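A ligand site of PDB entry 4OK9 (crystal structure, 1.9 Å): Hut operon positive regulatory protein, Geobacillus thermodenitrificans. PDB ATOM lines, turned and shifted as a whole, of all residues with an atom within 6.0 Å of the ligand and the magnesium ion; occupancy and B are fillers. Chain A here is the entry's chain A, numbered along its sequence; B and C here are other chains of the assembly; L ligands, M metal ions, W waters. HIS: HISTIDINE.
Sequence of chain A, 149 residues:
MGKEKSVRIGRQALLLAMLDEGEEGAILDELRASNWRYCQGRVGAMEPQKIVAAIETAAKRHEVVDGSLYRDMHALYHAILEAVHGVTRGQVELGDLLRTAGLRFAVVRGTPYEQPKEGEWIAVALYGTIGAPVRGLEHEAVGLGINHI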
ATOM      1  N   VAL A  87      38.221   0.223 -31.074  1.00  0.00           N
ATOM      2  CA  VAL A  87      37.089   0.348 -30.181  1.00  0.00           C
ATOM      3  C   VAL A  87      36.132  -0.849 -30.225  1.00  0.00           C
ATOM      4  O   VAL A  87      35.584  -1.236 -29.174  1.00  0.00           O
ATOM      5  CB  VAL A  87      36.298   1.678 -30.454  1.00  0.00           C
ATOM      6  CG1 VAL A  87      34.992   1.726 -29.722  1.00  0.00           C
ATOM      7  CG2 VAL A  87      37.147   2.863 -30.105  1.00  0.00           C
ATOM      8  N   THR A  88      35.896  -1.383 -31.386  1.00  0.00           N
ATOM      9  CA  THR A  88      34.927  -2.450 -31.493  1.00  0.00           C
ATOM     10  C   THR A  88      35.554  -3.859 -31.403  1.00  0.00           C
ATOM     11  O   THR A  88      34.864  -4.810 -31.249  1.00  0.00           O
ATOM     12  CB  THR A  88      34.087  -2.310 -32.750  1.00  0.00           C
ATOM     13  OG1 THR A  88      34.918  -2.245 -33.880  1.00  0.00           O
ATOM     14  CG2 THR A  88      33.286  -1.059 -32.694  1.00  0.00           C
ATOM     15  N   ARG A  89      36.859  -3.925 -31.486  1.00  0.00           N
ATOM     16  CA  ARG A  89      37.641  -5.120 -31.248  1.00  0.00           C
ATOM     17  C   ARG A  89      37.165  -6.293 -32.131  1.00  0.00           C
ATOM     18  O   ARG A  89      37.073  -7.408 -31.694  1.00  0.00           O
ATOM     19  CB  ARG A  89      37.649  -5.470 -29.764  1.00  0.00           C
ATOM     20  CG  ARG A  89      38.570  -4.606 -28.939  1.00  0.00           C
ATOM     21  CD  ARG A  89      37.964  -4.206 -27.584  1.00  0.00           C
ATOM     22  NE  ARG A  89      36.712  -3.517 -27.727  1.00  0.00           N
ATOM     23  CZ  ARG A  89      35.559  -3.950 -27.253  1.00  0.00           C
ATOM     24  NH1 ARG A  89      35.491  -5.056 -26.583  1.00  0.00           N
ATOM     25  NH2 ARG A  89      34.473  -3.280 -27.477  1.00  0.00           N
ATOM     26  N   LEU A  97      24.608  -4.669 -33.008  1.00  0.00           N
ATOM     27  CA  LEU A  97      24.954  -5.686 -32.039  1.00  0.00           C
ATOM     28  C   LEU A  97      24.476  -5.286 -30.623  1.00  0.00           C
ATOM     29  O   LEU A  97      25.007  -5.759 -29.583  1.00  0.00           O
ATOM     30  CB  LEU A  97      26.449  -5.992 -32.056  1.00  0.00           C
ATOM     31  CG  LEU A  97      26.962  -6.671 -33.366  1.00  0.00           C
ATOM     32  CD1 LEU A  97      28.444  -7.105 -33.217  1.00  0.00           C
ATOM     33  CD2 LEU A  97      26.107  -7.811 -33.765  1.00  0.00           C
ATOM     34  N   LEU A  98      23.511  -4.356 -30.574  1.00  0.00           N
ATOM     35  CA  LEU A  98      22.913  -3.908 -29.286  1.00  0.00           C
ATOM     36  C   LEU A  98      23.935  -3.332 -28.322  1.00  0.00           C
ATOM     37  O   LEU A  98      23.999  -3.736 -27.178  1.00  0.00           O
ATOM     38  CB  LEU A  98      22.207  -5.055 -28.618  1.00  0.00           C
ATOM     39  CG  LEU A  98      21.001  -4.650 -27.699  1.00  0.00           C
ATOM     40  CD1 LEU A  98      19.893  -4.074 -28.523  1.00  0.00           C
ATOM     41  CD2 LEU A  98      20.415  -5.849 -27.003  1.00  0.00           C
ATOM     42  N   ARG A  99      24.813  -2.450 -28.810  1.00  0.00           N
ATOM     43  CA  ARG A  99      25.713  -1.714 -27.970  1.00  0.00           C
ATOM     44  C   ARG A  99      25.805  -0.263 -28.502  1.00  0.00           C
ATOM     45  O   ARG A  99      25.374  -0.010 -29.608  1.00  0.00           O
ATOM     46  CB  ARG A  99      27.094  -2.331 -27.870  1.00  0.00           C
ATOM     47  CG  ARG A  99      27.945  -2.295 -29.083  1.00  0.00           C
ATOM     48  CD  ARG A  99      29.218  -3.156 -28.850  1.00  0.00           C
ATOM     49  NE  ARG A  99      29.800  -3.460 -30.147  1.00  0.00           N
ATOM     50  CZ  ARG A  99      30.797  -4.288 -30.379  1.00  0.00           C
ATOM     51  NH1 ARG A  99      31.360  -4.957 -29.368  1.00  0.00           N
ATOM     52  NH2 ARG A  99      31.217  -4.473 -31.632  1.00  0.00           N
ATOM     53  N   THR A 100      26.371   0.618 -27.695  1.00  0.00           N
ATOM     54  CA  THR A 100      26.427   2.056 -28.029  1.00  0.00           C
ATOM     55  C   THR A 100      27.750   2.459 -27.478  1.00  0.00           C
ATOM     56  O   THR A 100      28.329   1.755 -26.627  1.00  0.00           O
ATOM     57  CB  THR A 100      25.257   2.869 -27.372  1.00  0.00           C
ATOM     58  OG1 THR A 100      25.368   2.738 -25.988  1.00  0.00           O
ATOM     59  CG2 THR A 100      23.919   2.301 -27.659  1.00  0.00           C
ATOM     60  N   ILE A 130      32.082   1.740 -24.085  1.00  0.00           N
ATOM     61  CA  ILE A 130      31.185   0.970 -24.956  1.00  0.00           C
ATOM     62  C   ILE A 130      30.359   0.111 -24.080  1.00  0.00           C
ATOM     63  O   ILE A 130      30.866  -0.458 -23.081  1.00  0.00           O
ATOM     64  CB  ILE A 130      31.988   0.178 -26.012  1.00  0.00           C
ATOM     65  CG1 ILE A 130      31.047  -0.386 -27.085  1.00  0.00           C
ATOM     66  CG2 ILE A 130      32.887  -0.892 -25.387  1.00  0.00           C
ATOM     67  CD1 ILE A 130      31.791  -0.543 -28.367  1.00  0.00           C
ATOM     68  N   GLY A 131      29.125  -0.085 -24.428  1.00  0.00           N
ATOM     69  CA  GLY A 131      28.339  -0.802 -23.478  1.00  0.00           C
ATOM     70  C   GLY A 131      26.997  -1.025 -23.956  1.00  0.00           C
ATOM     71  O   GLY A 131      26.665  -0.709 -25.072  1.00  0.00           O
ATOM     72  N   ALA A 132      26.174  -1.520 -23.074  1.00  0.00           N
ATOM     73  CA  ALA A 132      24.799  -1.693 -23.328  1.00  0.00           C
ATOM     74  C   ALA A 132      24.131  -0.348 -23.448  1.00  0.00           C
ATOM     75  O   ALA A 132      24.608   0.625 -22.950  1.00  0.00           O
ATOM     76  CB  ALA A 132      24.148  -2.490 -22.239  1.00  0.00           C
ATOM     77  N   PRO A 133      22.920  -0.386 -24.146  1.00  0.00           N
ATOM     78  CA  PRO A 133      22.284   0.933 -24.292  1.00  0.00           C
ATOM     79  C   PRO A 133      21.809   1.559 -22.998  1.00  0.00           C
ATOM     80  O   PRO A 133      21.088   2.478 -23.082  1.00  0.00           O
ATOM     81  CB  PRO A 133      21.072   0.659 -25.153  1.00  0.00           C
ATOM     82  CG  PRO A 133      21.426  -0.504 -25.965  1.00  0.00           C
ATOM     83  CD  PRO A 133      22.086  -1.376 -24.986  1.00  0.00           C
ATOM     84  N   LEU A 137      26.181   0.179 -17.608  1.00  0.00           N
ATOM     85  CA  LEU A 137      26.513  -1.175 -18.064  1.00  0.00           C
ATOM     86  C   LEU A 137      27.460  -1.023 -19.281  1.00  0.00           C
ATOM     87  O   LEU A 137      27.034  -1.105 -20.435  1.00  0.00           O
ATOM     88  CB  LEU A 137      25.246  -1.916 -18.437  1.00  0.00           C
ATOM     89  CG  LEU A 137      24.140  -2.199 -17.431  1.00  0.00           C
ATOM     90  CD1 LEU A 137      23.077  -3.131 -18.033  1.00  0.00           C
ATOM     91  CD2 LEU A 137      24.736  -2.826 -16.199  1.00  0.00           C
ATOM     92  N   GLU A 138      28.689  -0.649 -18.991  1.00  0.00           N
ATOM     93  CA  GLU A 138      29.699  -0.292 -20.016  1.00  0.00           C
ATOM     94  C   GLU A 138      31.063  -0.467 -19.468  1.00  0.00           C
ATOM     95  O   GLU A 138      31.232  -0.494 -18.271  1.00  0.00           O
ATOM     96  CB  GLU A 138      29.494   1.160 -20.418  1.00  0.00           C
ATOM     97  CG  GLU A 138      29.788   2.109 -19.249  1.00  0.00           C
ATOM     98  CD  GLU A 138      29.051   3.400 -19.304  1.00  0.00           C
ATOM     99  OE1 GLU A 138      28.233   3.643 -20.235  1.00  0.00           O
ATOM    100  OE2 GLU A 138      29.291   4.140 -18.364  1.00  0.00           O
ATOM    101  N   HIS A 139      32.095  -0.583 -20.334  1.00  0.00           N
ATOM    102  CA  HIS A 139      33.487  -0.473 -19.963  1.00  0.00           C
ATOM    103  C   HIS A 139      34.228   0.339 -20.997  1.00  0.00           C
ATOM    104  O   HIS A 139      33.583   0.897 -21.934  1.00  0.00           O
ATOM    105  CB  HIS A 139      34.140  -1.856 -19.750  1.00  0.00           C
ATOM    106  CG  HIS A 139      34.063  -2.742 -20.982  1.00  0.00           C
ATOM    107  ND1 HIS A 139      34.764  -2.473 -22.142  1.00  0.00           N
ATOM    108  CD2 HIS A 139      33.385  -3.895 -21.198  1.00  0.00           C
ATOM    109  CE1 HIS A 139      34.532  -3.442 -23.018  1.00  0.00           C
ATOM    110  NE2 HIS A 139      33.716  -4.316 -22.464  1.00  0.00           N
ATOM    111  N   GLU B  56      18.829 -11.829 -24.176  1.00  0.00           N
ATOM    112  CA  GLU B  56      18.925 -11.024 -22.911  1.00  0.00           C
ATOM    113  C   GLU B  56      17.532 -11.020 -22.165  1.00  0.00           C
ATOM    114  O   GLU B  56      17.479 -11.194 -20.956  1.00  0.00           O
ATOM    115  CB  GLU B  56      19.426  -9.628 -23.244  1.00  0.00           C
ATOM    116  CG  GLU B  56      20.948  -9.499 -23.411  1.00  0.00           C
ATOM    117  CD  GLU B  56      21.441  -8.093 -23.680  1.00  0.00           C
ATOM    118  OE1 GLU B  56      20.652  -7.120 -23.465  1.00  0.00           O
ATOM    119  OE2 GLU B  56      22.623  -7.894 -24.047  1.00  0.00           O
ATOM    120  N   TYR B  70      26.386  -5.643 -14.082  1.00  0.00           N
ATOM    121  CA  TYR B  70      27.065  -5.602 -15.383  1.00  0.00           C
ATOM    122  C   TYR B  70      27.920  -6.848 -15.610  1.00  0.00           C
ATOM    123  O   TYR B  70      27.962  -7.292 -16.720  1.00  0.00           O
ATOM    124  CB  TYR B  70      27.906  -4.373 -15.572  1.00  0.00           C
ATOM    125  CG  TYR B  70      28.440  -4.211 -17.018  1.00  0.00           C
ATOM    126  CD1 TYR B  70      27.639  -4.418 -18.108  1.00  0.00           C
ATOM    127  CD2 TYR B  70      29.749  -3.896 -17.255  1.00  0.00           C
ATOM    128  CE1 TYR B  70      28.138  -4.288 -19.402  1.00  0.00           C
ATOM    129  CE2 TYR B  70      30.240  -3.722 -18.563  1.00  0.00           C
ATOM    130  CZ  TYR B  70      29.414  -3.913 -19.618  1.00  0.00           C
ATOM    131  OH  TYR B  70      29.892  -3.779 -20.954  1.00  0.00           O
ATOM    132  N   MET B  73      25.796  -9.349 -17.259  1.00  0.00           N
ATOM    133  CA  MET B  73      25.379  -8.986 -18.563  1.00  0.00           C
ATOM    134  C   MET B  73      26.555  -8.913 -19.556  1.00  0.00           C
ATOM    135  O   MET B  73      26.336  -9.173 -20.733  1.00  0.00           O
ATOM    136  CB  MET B  73      24.596  -7.667 -18.462  1.00  0.00           C
ATOM    137  CG  MET B  73      23.373  -7.858 -17.568  1.00  0.00           C
ATOM    138  SD  MET B  73      22.225  -9.169 -18.047  1.00  0.00           S
ATOM    139  CE  MET B  73      21.671  -8.675 -19.583  1.00  0.00           C
ATOM    140  N   HIS B  74      27.737  -8.626 -19.090  1.00  0.00           N
ATOM    141  CA  HIS B  74      28.954  -8.574 -19.896  1.00  0.00           C
ATOM    142  C   HIS B  74      29.322 -10.021 -20.318  1.00  0.00           C
ATOM    143  O   HIS B  74      29.615 -10.331 -21.498  1.00  0.00           O
ATOM    144  CB  HIS B  74      30.044  -8.024 -19.055  1.00  0.00           C
ATOM    145  CG  HIS B  74      31.302  -7.773 -19.838  1.00  0.00           C
ATOM    146  ND1 HIS B  74      32.233  -8.749 -20.171  1.00  0.00           N
ATOM    147  CD2 HIS B  74      31.854  -6.617 -20.194  1.00  0.00           C
ATOM    148  CE1 HIS B  74      33.253  -8.194 -20.783  1.00  0.00           C
ATOM    149  NE2 HIS B  74      33.045  -6.903 -20.829  1.00  0.00           N
ATOM    150  N   TYR B  77      26.568 -11.163 -22.796  1.00  0.00           N
ATOM    151  CA  TYR B  77      26.629 -10.486 -24.087  1.00  0.00           C
ATOM    152  C   TYR B  77      27.707 -11.152 -24.975  1.00  0.00           C
ATOM    153  O   TYR B  77      27.413 -11.399 -26.113  1.00  0.00           O
ATOM    154  CB  TYR B  77      26.991  -9.049 -23.912  1.00  0.00           C
ATOM    155  CG  TYR B  77      27.087  -8.277 -25.170  1.00  0.00           C
ATOM    156  CD1 TYR B  77      25.980  -7.922 -25.831  1.00  0.00           C
ATOM    157  CD2 TYR B  77      28.327  -7.953 -25.698  1.00  0.00           C
ATOM    158  CE1 TYR B  77      26.038  -7.210 -27.040  1.00  0.00           C
ATOM    159  CE2 TYR B  77      28.420  -7.240 -26.882  1.00  0.00           C
ATOM    160  CZ  TYR B  77      27.291  -6.881 -27.548  1.00  0.00           C
ATOM    161  OH  TYR B  77      27.416  -6.214 -28.770  1.00  0.00           O
ATOM    162  N   HIS B  78      28.902 -11.370 -24.408  1.00  0.00           N
ATOM    163  CA  HIS B  78      30.031 -11.950 -25.178  1.00  0.00           C
ATOM    164  C   HIS B  78      29.730 -13.336 -25.617  1.00  0.00           C
ATOM    165  O   HIS B  78      30.100 -13.727 -26.703  1.00  0.00           O
ATOM    166  CB  HIS B  78      31.381 -11.781 -24.448  1.00  0.00           C
ATOM    167  CG  HIS B  78      31.889 -10.366 -24.583  1.00  0.00           C
ATOM    168  ND1 HIS B  78      32.418  -9.881 -25.757  1.00  0.00           N
ATOM    169  CD2 HIS B  78      31.919  -9.342 -23.729  1.00  0.00           C
ATOM    170  CE1 HIS B  78      32.769  -8.614 -25.612  1.00  0.00           C
ATOM    171  NE2 HIS B  78      32.441  -8.263 -24.386  1.00  0.00           N
ATOM    172  N   GLU C  82      41.418  -9.025 -27.564  1.00  0.00           N
ATOM    173  CA  GLU C  82      40.841  -7.653 -27.803  1.00  0.00           C
ATOM    174  C   GLU C  82      41.847  -6.536 -27.958  1.00  0.00           C
ATOM    175  O   GLU C  82      41.750  -5.647 -28.868  1.00  0.00           O
ATOM    176  CB  GLU C  82      39.816  -7.348 -26.702  1.00  0.00           C
ATOM    177  CG  GLU C  82      38.491  -8.168 -26.656  1.00  0.00           C
ATOM    178  CD  GLU C  82      37.539  -7.597 -25.604  1.00  0.00           C
ATOM    179  OE1 GLU C  82      37.995  -6.669 -24.860  1.00  0.00           O
ATOM    180  OE2 GLU C  82      36.323  -7.957 -25.539  1.00  0.00           O
ATOM    181  N   ILE C 146      39.209  -5.306 -22.177  1.00  0.00           N
ATOM    182  CA  ILE C 146      38.682  -5.348 -20.830  1.00  0.00           C
ATOM    183  C   ILE C 146      37.867  -6.593 -20.676  1.00  0.00           C
ATOM    184  O   ILE C 146      36.959  -6.888 -21.493  1.00  0.00           O
ATOM    185  CB  ILE C 146      37.687  -4.139 -20.630  1.00  0.00           C
ATOM    186  CG1 ILE C 146      38.416  -2.785 -20.765  1.00  0.00           C
ATOM    187  CG2 ILE C 146      36.944  -4.148 -19.285  1.00  0.00           C
ATOM    188  CD1 ILE C 146      39.548  -2.542 -19.807  1.00  0.00           C
ATOM    189  N   ASN C 147      38.019  -7.272 -19.524  1.00  0.00           N
ATOM    190  CA  ASN C 147      37.091  -8.334 -19.197  1.00  0.00           C
ATOM    191  C   ASN C 147      36.783  -8.452 -17.675  1.00  0.00           C
ATOM    192  O   ASN C 147      37.526  -7.988 -16.873  1.00  0.00           O
ATOM    193  CB  ASN C 147      37.706  -9.651 -19.681  1.00  0.00           C
ATOM    194  CG  ASN C 147      36.682 -10.668 -20.122  1.00  0.00           C
ATOM    195  OD1 ASN C 147      35.487 -10.503 -20.085  1.00  0.00           O
ATOM    196  ND2 ASN C 147      37.223 -11.820 -20.562  1.00  0.00           N
HETATM  197  N   HIS L   1      30.973  -5.518 -23.446  1.00  0.00           N
HETATM  198  CA  HIS L   1      30.633  -5.150 -24.865  1.00  0.00           C
HETATM  199  C   HIS L   1      31.892  -4.858 -25.612  1.00  0.00           C
HETATM  200  O   HIS L   1      31.883  -4.171 -26.618  1.00  0.00           O
HETATM  201  CB  HIS L   1      29.652  -3.981 -24.853  1.00  0.00           C
HETATM  202  CG  HIS L   1      28.323  -4.354 -24.304  1.00  0.00           C
HETATM  203  ND1 HIS L   1      28.100  -4.570 -22.952  1.00  0.00           N
HETATM  204  CD2 HIS L   1      27.140  -4.611 -24.911  1.00  0.00           C
HETATM  205  CE1 HIS L   1      26.872  -4.983 -22.777  1.00  0.00           C
HETATM  206  NE2 HIS L   1      26.257  -4.990 -23.935  1.00  0.00           N
HETATM  207  OXT HIS L   1      33.019  -5.288 -25.257  1.00  0.00           O
HETATM  208 MG    MG M   1      33.163  -6.334 -23.406  1.00  0.00          MG
HETATM  209  O   HOH W   1      23.527  -5.300 -24.867  1.00  0.00           O
HETATM  210  O   HOH W   2      35.050  -6.790 -23.530  1.00  0.00           O
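The magnesium ion is bound by water W2 (1.9 Å), OXT of the ligand (2.1 Å), NE2 of His 78 of chain B (2.3 Å), NE2 of His 139 (2.3 Å) and N of the ligand (2.3 Å). The magnesium ion has five donor atoms within binding distance. Slightly farther from the magnesium ion lies NE2 of His 74 of chain B (2.6 Å).
A ring nitrogen (NE2) of His 74 of chain B lies close to a ring nitrogen (NE2) of His 139 (3.1 Å). O of His 139 sits at hydrogen-bond distance from N of Ile 130. The side-chain carboxylate of Glu 82 of chain C is in salt-bridge range of the guanidinium group of Arg 89, 3.2 Å away. NH2 of Arg 89 sits at hydrogen-bond distance from O of Val 87 (2.9 Å). The backbone carbonyl oxygen (O) of Leu 97 sits at hydrogen-bond distance from the side-chain hydroxyl (OH) of Tyr 77 of chain B (2.6 Å). The backbone NH of Ala 132 lies within hydrogen-bond range of the backbone carbonyl oxygen of Leu 137. The backbone carbonyl oxygen (O) of Gly 131 sits at hydrogen-bond distance from the backbone NH (N) of Thr 100 (3.0 Å).
Three residues have an atom within 4 Å of the magnesium ion: His 139, His 74 of chain B and His 78 of chain B. The nearest printed residue that does not touch the magnesium ion is Arg 89 (4.1 Å).
ND1 of the ligand lies within hydrogen-bond range of OH of Tyr 70 of chain B (2.8 Å). NH2 of Arg 89 lies within salt-bridge range of O of the ligand, 2.9 Å away. An oxygen (O) of the ligand is in salt-bridge range of the guanidinium group (NH1) of Arg 99 (2.9 Å).
Leu 98 touches the ligand. Ile 130 touches the ligand. C of Gly 131 touches CG of the ligand, at 3.6 Å. N of Ala 132 touches CE1 of the ligand (3.5 Å). Tyr 77 of chain B touches the ligand (CZ to CD2, 3.5 Å). Hydrophobic or aromatic side chains that line the ligand: Ile 130, Ala 132, His 139, Tyr 70 of chain B, His 74 of chain B, Tyr 77 of chain B and His 78 of chain B. 11 residues have an atom within 4 Å of the ligand: Arg 89, Leu 98, Arg 99, Ile 130, Gly 131, Ala 132, His 139, Tyr 70 of chain B, His 74 of chain B, Tyr 77 of chain B and His 78 of chain B. Along chain A the residues within 4 Å of the ligand span positions 89 to 139. The nearest printed residue that does not touch the ligand is Glu 82 of chain C (4.3 Å).
Water W2 lies within hydrogen-bond range of the side-chain carboxylate of Glu 82 of chain C (2.6 Å), the backbone carbonyl oxygen of Ile 146 of chain C (2.8 Å) and a ring nitrogen (NE2) of His 74 of chain B (3.4 Å). Water W1 lies within hydrogen-bond range of the backbone carbonyl oxygen of Leu 98 (2.8 Å), the side-chain carboxylate of Glu 56 of chain B (2.9 Å) and a nitrogen (NE2) of the ligand (2.9 Å).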
